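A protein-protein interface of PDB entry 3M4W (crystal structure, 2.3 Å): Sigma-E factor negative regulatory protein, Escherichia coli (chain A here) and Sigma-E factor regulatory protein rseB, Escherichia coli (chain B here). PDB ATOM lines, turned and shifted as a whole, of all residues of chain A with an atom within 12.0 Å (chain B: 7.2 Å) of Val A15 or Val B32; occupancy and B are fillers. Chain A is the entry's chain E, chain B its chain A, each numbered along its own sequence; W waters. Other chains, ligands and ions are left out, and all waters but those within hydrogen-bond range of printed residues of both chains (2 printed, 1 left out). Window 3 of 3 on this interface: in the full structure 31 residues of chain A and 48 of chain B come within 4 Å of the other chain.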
ATOM      1  N   GLU A  12     -35.856 -21.731  -5.455  1.00  0.00           N
ATOM      2  CA  GLU A  12     -35.166 -21.482  -4.159  1.00  0.00           C
ATOM      3  C   GLU A  12     -35.736 -22.239  -2.965  1.00  0.00           C
ATOM      4  O   GLU A  12     -36.771 -21.867  -2.406  1.00  0.00           O
ATOM      5  CB  GLU A  12     -35.158 -19.983  -3.820  1.00  0.00           C
ATOM      6  CG  GLU A  12     -35.019 -19.691  -2.316  1.00  0.00           C
ATOM      7  CD  GLU A  12     -35.105 -18.215  -1.971  1.00  0.00           C
ATOM      8  OE1 GLU A  12     -35.903 -17.497  -2.613  1.00  0.00           O
ATOM      9  OE2 GLU A  12     -34.385 -17.777  -1.044  1.00  0.00           O
ATOM     10  N   THR A  13     -35.064 -23.323  -2.607  1.00  0.00           N
ATOM     11  CA  THR A  13     -35.406 -24.093  -1.427  1.00  0.00           C
ATOM     12  C   THR A  13     -34.098 -23.747  -0.744  1.00  0.00           C
ATOM     13  O   THR A  13     -33.059 -24.309  -1.082  1.00  0.00           O
ATOM     14  CB  THR A  13     -35.451 -25.616  -1.686  1.00  0.00           C
ATOM     15  OG1 THR A  13     -36.303 -25.897  -2.805  1.00  0.00           O
ATOM     16  CG2 THR A  13     -35.984 -26.341  -0.450  1.00  0.00           C
ATOM     17  N   PRO A  14     -34.121 -22.793   0.198  1.00  0.00           N
ATOM     18  CA  PRO A  14     -32.872 -22.418   0.871  1.00  0.00           C
ATOM     19  C   PRO A  14     -31.878 -23.566   1.036  1.00  0.00           C
ATOM     20  O   PRO A  14     -30.674 -23.399   0.848  1.00  0.00           O
ATOM     21  CB  PRO A  14     -33.356 -21.856   2.216  1.00  0.00           C
ATOM     22  CG  PRO A  14     -34.687 -22.532   2.429  1.00  0.00           C
ATOM     23  CD  PRO A  14     -35.280 -22.449   1.040  1.00  0.00           C
ATOM     24  N   VAL A  15     -32.404 -24.742   1.346  1.00  0.00           N
ATOM     25  CA  VAL A  15     -31.586 -25.922   1.585  1.00  0.00           C
ATOM     26  C   VAL A  15     -30.579 -26.360   0.513  1.00  0.00           C
ATOM     27  O   VAL A  15     -29.492 -26.798   0.854  1.00  0.00           O
ATOM     28  CB  VAL A  15     -32.483 -27.139   1.917  1.00  0.00           C
ATOM     29  CG1 VAL A  15     -31.920 -27.876   3.122  1.00  0.00           C
ATOM     30  CG2 VAL A  15     -33.907 -26.681   2.195  1.00  0.00           C
ATOM     31  N   PHE A  16     -30.933 -26.246  -0.768  1.00  0.00           N
ATOM     32  CA  PHE A  16     -30.057 -26.707  -1.846  1.00  0.00           C
ATOM     33  C   PHE A  16     -29.175 -25.657  -2.469  1.00  0.00           C
ATOM     34  O   PHE A  16     -28.388 -25.971  -3.361  1.00  0.00           O
ATOM     35  CB  PHE A  16     -30.885 -27.354  -2.957  1.00  0.00           C
ATOM     36  CG  PHE A  16     -31.715 -28.497  -2.492  1.00  0.00           C
ATOM     37  CD1 PHE A  16     -33.039 -28.618  -2.898  1.00  0.00           C
ATOM     38  CD2 PHE A  16     -31.180 -29.455  -1.644  1.00  0.00           C
ATOM     39  CE1 PHE A  16     -33.833 -29.676  -2.440  1.00  0.00           C
ATOM     40  CE2 PHE A  16     -31.958 -30.513  -1.183  1.00  0.00           C
ATOM     41  CZ  PHE A  16     -33.288 -30.629  -1.588  1.00  0.00           C
ATOM     42  N   ASN A  17     -29.321 -24.411  -2.025  1.00  0.00           N
ATOM     43  CA  ASN A  17     -28.516 -23.307  -2.547  1.00  0.00           C
ATOM     44  C   ASN A  17     -27.188 -23.322  -1.802  1.00  0.00           C
ATOM     45  O   ASN A  17     -27.147 -23.071  -0.607  1.00  0.00           O
ATOM     46  CB  ASN A  17     -29.246 -21.968  -2.335  1.00  0.00           C
ATOM     47  CG  ASN A  17     -28.416 -20.768  -2.782  1.00  0.00           C
ATOM     48  OD1 ASN A  17     -27.436 -20.908  -3.514  1.00  0.00           O
ATOM     49  ND2 ASN A  17     -28.815 -19.583  -2.349  1.00  0.00           N
ATOM     50  N   THR A  18     -26.105 -23.613  -2.510  1.00  0.00           N
ATOM     51  CA  THR A  18     -24.791 -23.703  -1.880  1.00  0.00           C
ATOM     52  C   THR A  18     -23.995 -22.409  -1.859  1.00  0.00           C
ATOM     53  O   THR A  18     -23.013 -22.304  -1.131  1.00  0.00           O
ATOM     54  CB  THR A  18     -23.931 -24.760  -2.570  1.00  0.00           C
ATOM     55  OG1 THR A  18     -23.415 -24.212  -3.781  1.00  0.00           O
ATOM     56  CG2 THR A  18     -24.751 -25.972  -2.922  1.00  0.00           C
ATOM     57  N   LEU A  19     -24.409 -21.437  -2.666  1.00  0.00           N
ATOM     58  CA  LEU A  19     -23.722 -20.151  -2.748  1.00  0.00           C
ATOM     59  C   LEU A  19     -24.683 -19.049  -2.342  1.00  0.00           C
ATOM     60  O   LEU A  19     -25.161 -18.287  -3.179  1.00  0.00           O
ATOM     61  CB  LEU A  19     -23.233 -19.904  -4.178  1.00  0.00           C
ATOM     62  CG  LEU A  19     -22.215 -20.907  -4.727  1.00  0.00           C
ATOM     63  CD1 LEU A  19     -21.857 -20.550  -6.167  1.00  0.00           C
ATOM     64  CD2 LEU A  19     -20.974 -20.898  -3.848  1.00  0.00           C
ATOM     65  N   PRO A  20     -24.973 -18.944  -1.040  1.00  0.00           N
ATOM     66  CA  PRO A  20     -25.892 -17.931  -0.511  1.00  0.00           C
ATOM     67  C   PRO A  20     -25.492 -16.491  -0.804  1.00  0.00           C
ATOM     68  O   PRO A  20     -24.306 -16.169  -0.883  1.00  0.00           O
ATOM     69  CB  PRO A  20     -25.900 -18.230   0.984  1.00  0.00           C
ATOM     70  CG  PRO A  20     -24.506 -18.728   1.217  1.00  0.00           C
ATOM     71  CD  PRO A  20     -24.316 -19.672   0.058  1.00  0.00           C
ATOM     72  N   MET A  21     -26.494 -15.631  -0.960  1.00  0.00           N
ATOM     73  CA  MET A  21     -26.253 -14.223  -1.220  1.00  0.00           C
ATOM     74  C   MET A  21     -25.620 -13.622   0.029  1.00  0.00           C
ATOM     75  O   MET A  21     -26.138 -13.774   1.135  1.00  0.00           O
ATOM     76  CB  MET A  21     -27.563 -13.499  -1.539  1.00  0.00           C
ATOM     77  CG  MET A  21     -27.380 -12.032  -1.913  1.00  0.00           C
ATOM     78  SD  MET A  21     -28.939 -11.160  -2.245  1.00  0.00           S
ATOM     79  CE  MET A  21     -28.999 -10.007  -0.841  1.00  0.00           C
ATOM     80  N   MET A  22     -24.490 -12.953  -0.165  1.00  0.00           N
ATOM     81  CA  MET A  22     -23.753 -12.313   0.915  1.00  0.00           C
ATOM     82  C   MET A  22     -23.192 -13.315   1.919  1.00  0.00           C
ATOM     83  O   MET A  22     -23.496 -13.250   3.113  1.00  0.00           O
ATOM     84  CB  MET A  22     -24.631 -11.288   1.643  1.00  0.00           C
ATOM     85  CG  MET A  22     -23.828 -10.200   2.366  1.00  0.00           C
ATOM     86  SD  MET A  22     -23.281  -8.823   1.292  1.00  0.00           S
ATOM     87  CE  MET A  22     -22.254  -9.668   0.067  1.00  0.00           C
ATOM     88  N   GLY A  23     -22.366 -14.237   1.424  1.00  0.00           N
ATOM     89  CA  GLY A  23     -21.754 -15.233   2.283  1.00  0.00           C
ATOM     90  C   GLY A  23     -20.910 -14.590   3.370  1.00  0.00           C
ATOM     91  O   GLY A  23     -20.631 -13.393   3.323  1.00  0.00           O
ATOM     92  N   LYS A  24     -20.488 -15.394   4.342  1.00  0.00           N
ATOM     93  CA  LYS A  24     -19.692 -14.923   5.466  1.00  0.00           C
ATOM     94  C   LYS A  24     -18.345 -14.300   5.104  1.00  0.00           C
ATOM     95  O   LYS A  24     -17.835 -13.452   5.844  1.00  0.00           O
ATOM     96  CB  LYS A  24     -19.457 -16.073   6.453  1.00  0.00           C
ATOM     97  CG  LYS A  24     -20.727 -16.623   7.076  1.00  0.00           C
ATOM     98  CD  LYS A  24     -21.346 -15.605   8.007  1.00  0.00           C
ATOM     99  CE  LYS A  24     -22.583 -16.158   8.695  1.00  0.00           C
ATOM    100  NZ  LYS A  24     -22.946 -15.304   9.878  1.00  0.00           N
ATOM    101  N   ALA A  25     -17.767 -14.711   3.978  1.00  0.00           N
ATOM    102  CA  ALA A  25     -16.469 -14.179   3.578  1.00  0.00           C
ATOM    103  C   ALA A  25     -16.531 -13.018   2.589  1.00  0.00           C
ATOM    104  O   ALA A  25     -15.493 -12.565   2.104  1.00  0.00           O
ATOM    105  CB  ALA A  25     -15.595 -15.299   3.018  1.00  0.00           C
ATOM    106  N   ILE B  25     -20.177 -25.408   8.169  1.00  0.00           N
ATOM    107  CA  ILE B  25     -21.197 -24.892   7.282  1.00  0.00           C
ATOM    108  C   ILE B  25     -21.962 -23.804   8.012  1.00  0.00           C
ATOM    109  O   ILE B  25     -22.002 -23.764   9.240  1.00  0.00           O
ATOM    110  CB  ILE B  25     -22.177 -25.995   6.783  1.00  0.00           C
ATOM    111  CG1 ILE B  25     -22.869 -26.673   7.963  1.00  0.00           C
ATOM    112  CG2 ILE B  25     -21.414 -27.015   5.930  1.00  0.00           C
ATOM    113  CD1 ILE B  25     -23.868 -27.692   7.548  1.00  0.00           C
ATOM    114  N   SER B  26     -22.516 -22.882   7.242  1.00  0.00           N
ATOM    115  CA  SER B  26     -23.313 -21.787   7.785  1.00  0.00           C
ATOM    116  C   SER B  26     -24.659 -21.907   7.097  1.00  0.00           C
ATOM    117  O   SER B  26     -24.770 -21.759   5.874  1.00  0.00           O
ATOM    118  CB  SER B  26     -22.663 -20.440   7.475  1.00  0.00           C
ATOM    119  OG  SER B  26     -23.436 -19.386   8.016  1.00  0.00           O
ATOM    120  N   ILE B  27     -25.674 -22.182   7.902  1.00  0.00           N
ATOM    121  CA  ILE B  27     -27.024 -22.402   7.429  1.00  0.00           C
ATOM    122  C   ILE B  27     -28.021 -21.314   7.802  1.00  0.00           C
ATOM    123  O   ILE B  27     -28.163 -20.973   8.968  1.00  0.00           O
ATOM    124  CB  ILE B  27     -27.533 -23.768   7.995  1.00  0.00           C
ATOM    125  CG1 ILE B  27     -26.564 -24.871   7.566  1.00  0.00           C
ATOM    126  CG2 ILE B  27     -28.972 -24.083   7.522  1.00  0.00           C
ATOM    127  CD1 ILE B  27     -26.980 -26.238   8.037  1.00  0.00           C
ATOM    128  N   ASN B  28     -28.695 -20.758   6.802  1.00  0.00           N
ATOM    129  CA  ASN B  28     -29.736 -19.764   7.044  1.00  0.00           C
ATOM    130  C   ASN B  28     -30.735 -19.862   5.905  1.00  0.00           C
ATOM    131  O   ASN B  28     -30.742 -20.856   5.177  1.00  0.00           O
ATOM    132  CB  ASN B  28     -29.176 -18.333   7.175  1.00  0.00           C
ATOM    133  CG  ASN B  28     -28.344 -17.899   5.979  1.00  0.00           C
ATOM    134  OD1 ASN B  28     -28.662 -18.201   4.824  1.00  0.00           O
ATOM    135  ND2 ASN B  28     -27.277 -17.167   6.256  1.00  0.00           N
ATOM    136  N   LYS B  29     -31.582 -18.852   5.743  1.00  0.00           N
ATOM    137  CA  LYS B  29     -32.580 -18.883   4.677  1.00  0.00           C
ATOM    138  C   LYS B  29     -32.017 -18.670   3.271  1.00  0.00           C
ATOM    139  O   LYS B  29     -32.692 -18.949   2.281  1.00  0.00           O
ATOM    140  CB  LYS B  29     -33.682 -17.857   4.959  1.00  0.00           C
ATOM    141  CG  LYS B  29     -34.505 -18.170   6.208  1.00  0.00           C
ATOM    142  CD  LYS B  29     -35.154 -19.554   6.132  1.00  0.00           C
ATOM    143  CE  LYS B  29     -35.915 -19.886   7.416  1.00  0.00           C
ATOM    144  NZ  LYS B  29     -36.967 -18.871   7.733  1.00  0.00           N
ATOM    145  N   GLN B  30     -30.792 -18.165   3.171  1.00  0.00           N
ATOM    146  CA  GLN B  30     -30.194 -17.966   1.852  1.00  0.00           C
ATOM    147  C   GLN B  30     -29.574 -19.279   1.347  1.00  0.00           C
ATOM    148  O   GLN B  30     -29.304 -19.418   0.156  1.00  0.00           O
ATOM    149  CB  GLN B  30     -29.095 -16.885   1.885  1.00  0.00           C
ATOM    150  CG  GLN B  30     -29.555 -15.451   2.160  1.00  0.00           C
ATOM    151  CD  GLN B  30     -29.740 -15.161   3.635  1.00  0.00           C
ATOM    152  OE1 GLN B  30     -30.848 -15.262   4.171  1.00  0.00           O
ATOM    153  NE2 GLN B  30     -28.647 -14.806   4.309  1.00  0.00           N
ATOM    154  N   GLY B  31     -29.333 -20.226   2.260  1.00  0.00           N
ATOM    155  CA  GLY B  31     -28.749 -21.502   1.869  1.00  0.00           C
ATOM    156  C   GLY B  31     -27.760 -22.112   2.851  1.00  0.00           C
ATOM    157  O   GLY B  31     -27.719 -21.752   4.033  1.00  0.00           O
ATOM    158  N   VAL B  32     -26.949 -23.039   2.343  1.00  0.00           N
ATOM    159  CA  VAL B  32     -25.949 -23.735   3.142  1.00  0.00           C
ATOM    160  C   VAL B  32     -24.553 -23.431   2.596  1.00  0.00           C
ATOM    161  O   VAL B  32     -24.171 -23.882   1.526  1.00  0.00           O
ATOM    162  CB  VAL B  32     -26.210 -25.245   3.102  1.00  0.00           C
ATOM    163  CG1 VAL B  32     -25.181 -25.973   3.959  1.00  0.00           C
ATOM    164  CG2 VAL B  32     -27.645 -25.527   3.564  1.00  0.00           C
ATOM    165  N   GLU B  33     -23.784 -22.675   3.358  1.00  0.00           N
ATOM    166  CA  GLU B  33     -22.469 -22.267   2.924  1.00  0.00           C
ATOM    167  C   GLU B  33     -21.344 -23.050   3.591  1.00  0.00           C
ATOM    168  O   GLU B  33     -21.305 -23.225   4.807  1.00  0.00           O
ATOM    169  CB  GLU B  33     -22.311 -20.746   3.154  1.00  0.00           C
ATOM    170  CG  GLU B  33     -20.943 -20.179   2.767  1.00  0.00           C
ATOM    171  CD  GLU B  33     -20.901 -18.642   2.724  1.00  0.00           C
ATOM    172  OE1 GLU B  33     -21.404 -17.985   3.666  1.00  0.00           O
ATOM    173  OE2 GLU B  33     -20.351 -18.093   1.740  1.00  0.00           O
ATOM    174  N   SER B  34     -20.450 -23.527   2.749  1.00  0.00           N
ATOM    175  CA  SER B  34     -19.287 -24.301   3.141  1.00  0.00           C
ATOM    176  C   SER B  34     -18.142 -23.323   3.385  1.00  0.00           C
ATOM    177  O   SER B  34     -17.759 -22.550   2.489  1.00  0.00           O
ATOM    178  CB  SER B  34     -18.940 -25.269   2.008  1.00  0.00           C
ATOM    179  OG  SER B  34     -17.777 -25.996   2.300  1.00  0.00           O
ATOM    180  N   ASP B  54     -16.587 -22.890  -1.772  1.00  0.00           N
ATOM    181  CA  ASP B  54     -17.111 -23.112  -3.116  1.00  0.00           C
ATOM    182  C   ASP B  54     -17.268 -21.804  -3.901  1.00  0.00           C
ATOM    183  O   ASP B  54     -17.536 -20.737  -3.331  1.00  0.00           O
ATOM    184  CB  ASP B  54     -18.485 -23.802  -3.096  1.00  0.00           C
ATOM    185  CG  ASP B  54     -18.544 -25.039  -2.185  1.00  0.00           C
ATOM    186  OD1 ASP B  54     -17.545 -25.774  -2.032  1.00  0.00           O
ATOM    187  OD2 ASP B  54     -19.638 -25.283  -1.641  1.00  0.00           O
HETATM  188  O   HOH W   1     -18.742 -16.185   1.559  1.00  0.00           O
HETATM  189  O   HOH W   2     -20.870 -23.457  -0.089  1.00  0.00           O
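The backbone carbonyl oxygen (O) of Gln B30 sits at hydrogen-bond distance from the side-chain amide nitrogen (ND2) of Asn A17 (2.6 Å). The backbone NH (N) of Val B32 is in hydrogen-bond range of the backbone carbonyl oxygen (O) of Asn A17 (3.0 Å). The side-chain carboxylate (OE1) of Glu B33 lies within hydrogen-bond range of the backbone NH (N) of Lys A24, at 2.8 Å. The backbone carbonyl oxygen (O) of Thr A18 lies close to the backbone carbonyl oxygen (O) of Val B32 (3.3 Å).
Among the printed residues, pairs that only touch across the chains: Glu A12 with Lys B29 (3.9 Å), Pro A14 with Lys B29 (3.0 Å), Pro A14 with Gly B31 (2.9 Å), Val A15 with Val B32 (3.5 Å), Asn A17 with Gly B31 (3.3 Å), Leu A19 with Asp B54 (3.5 Å), Pro A20 with Gln B30 (3.6 Å), Pro A20 with Glu B33 (3.6 Å), Met A21 with Gln B30 (3.9 Å), Gly A23 with Glu B33 (3.1 Å) and Lys A24 with Ser B26 (3.4 Å).
Hydrophobic or aromatic side chains of chain B that line the printed part of chain A: Val B32. Among the printed residues, no Asp or Glu carboxylate lies within 4 Å of a Lys or Arg side-chain nitrogen of the other chain.
N of Ser B26 sits at hydrogen-bond distance from O of Glu B33 (2.7 Å). The backbone NH (N) of Gln B30 is in hydrogen-bond range of the side-chain amide oxygen (OD1) of Asn B28 (2.7 Å). OD1 of Asn B28 lies within hydrogen-bond range of N of Gly B31 (3.3 Å). OD1 of Asn A17 sits at hydrogen-bond distance from N of Leu A19.
Water W1 lies within hydrogen-bond range of OE2 of Glu B33 (2.5 Å), N of Ala A25 (3.0 Å) and N of Lys A24 (3.4 Å). Water W2 lies within hydrogen-bond range of O of Thr A18 (2.6 Å), OD2 of Asp B54 (2.7 Å) and N of Ser B34 (2.9 Å).
Of the printed residues of chain B, Glu A12 touches Lys B29 (3.9 Å). Printed residues of chain B within 4 Å of Pro A14: Lys B29 and Gly B31. Val A15 touches just one residue of chain B: Val B32 (3.5 Å). Phe A16 touches none of the printed residues of chain B. Printed residues of chain B within 4 Å of Asn A17: Gln B30, Gly B31 and Val B32. Of the printed residues of chain B, Thr A18 touches Val B32. Printed residues of chain B within 4 Å of Gly A23: Glu B33 (3.1 Å). Ala A25 touches none of the printed residues of chain B. No residue of chain A comes within 4 Å of Ile B25. Ile B27 touches none of the printed residues of chain A. No residue of chain A comes within 4 Å of Asn B28. Gly B31 touches two residues of chain A. Val B32 touches just these residues of chain A: Val A15, Asn A17 and Thr A18. Glu B33 touches three residues of chain A. No residue of chain A comes within 4 Å of Ser B34. The nearest residue of chain B that does not touch Val A15 is Gly B31 (4.9 Å). The nearest residue of chain A that does not touch Val B32 is Pro A14 (4.03 Å). The nearest printed residue of chain B that does not touch Met A21 is Asn B28 (6.2 Å).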
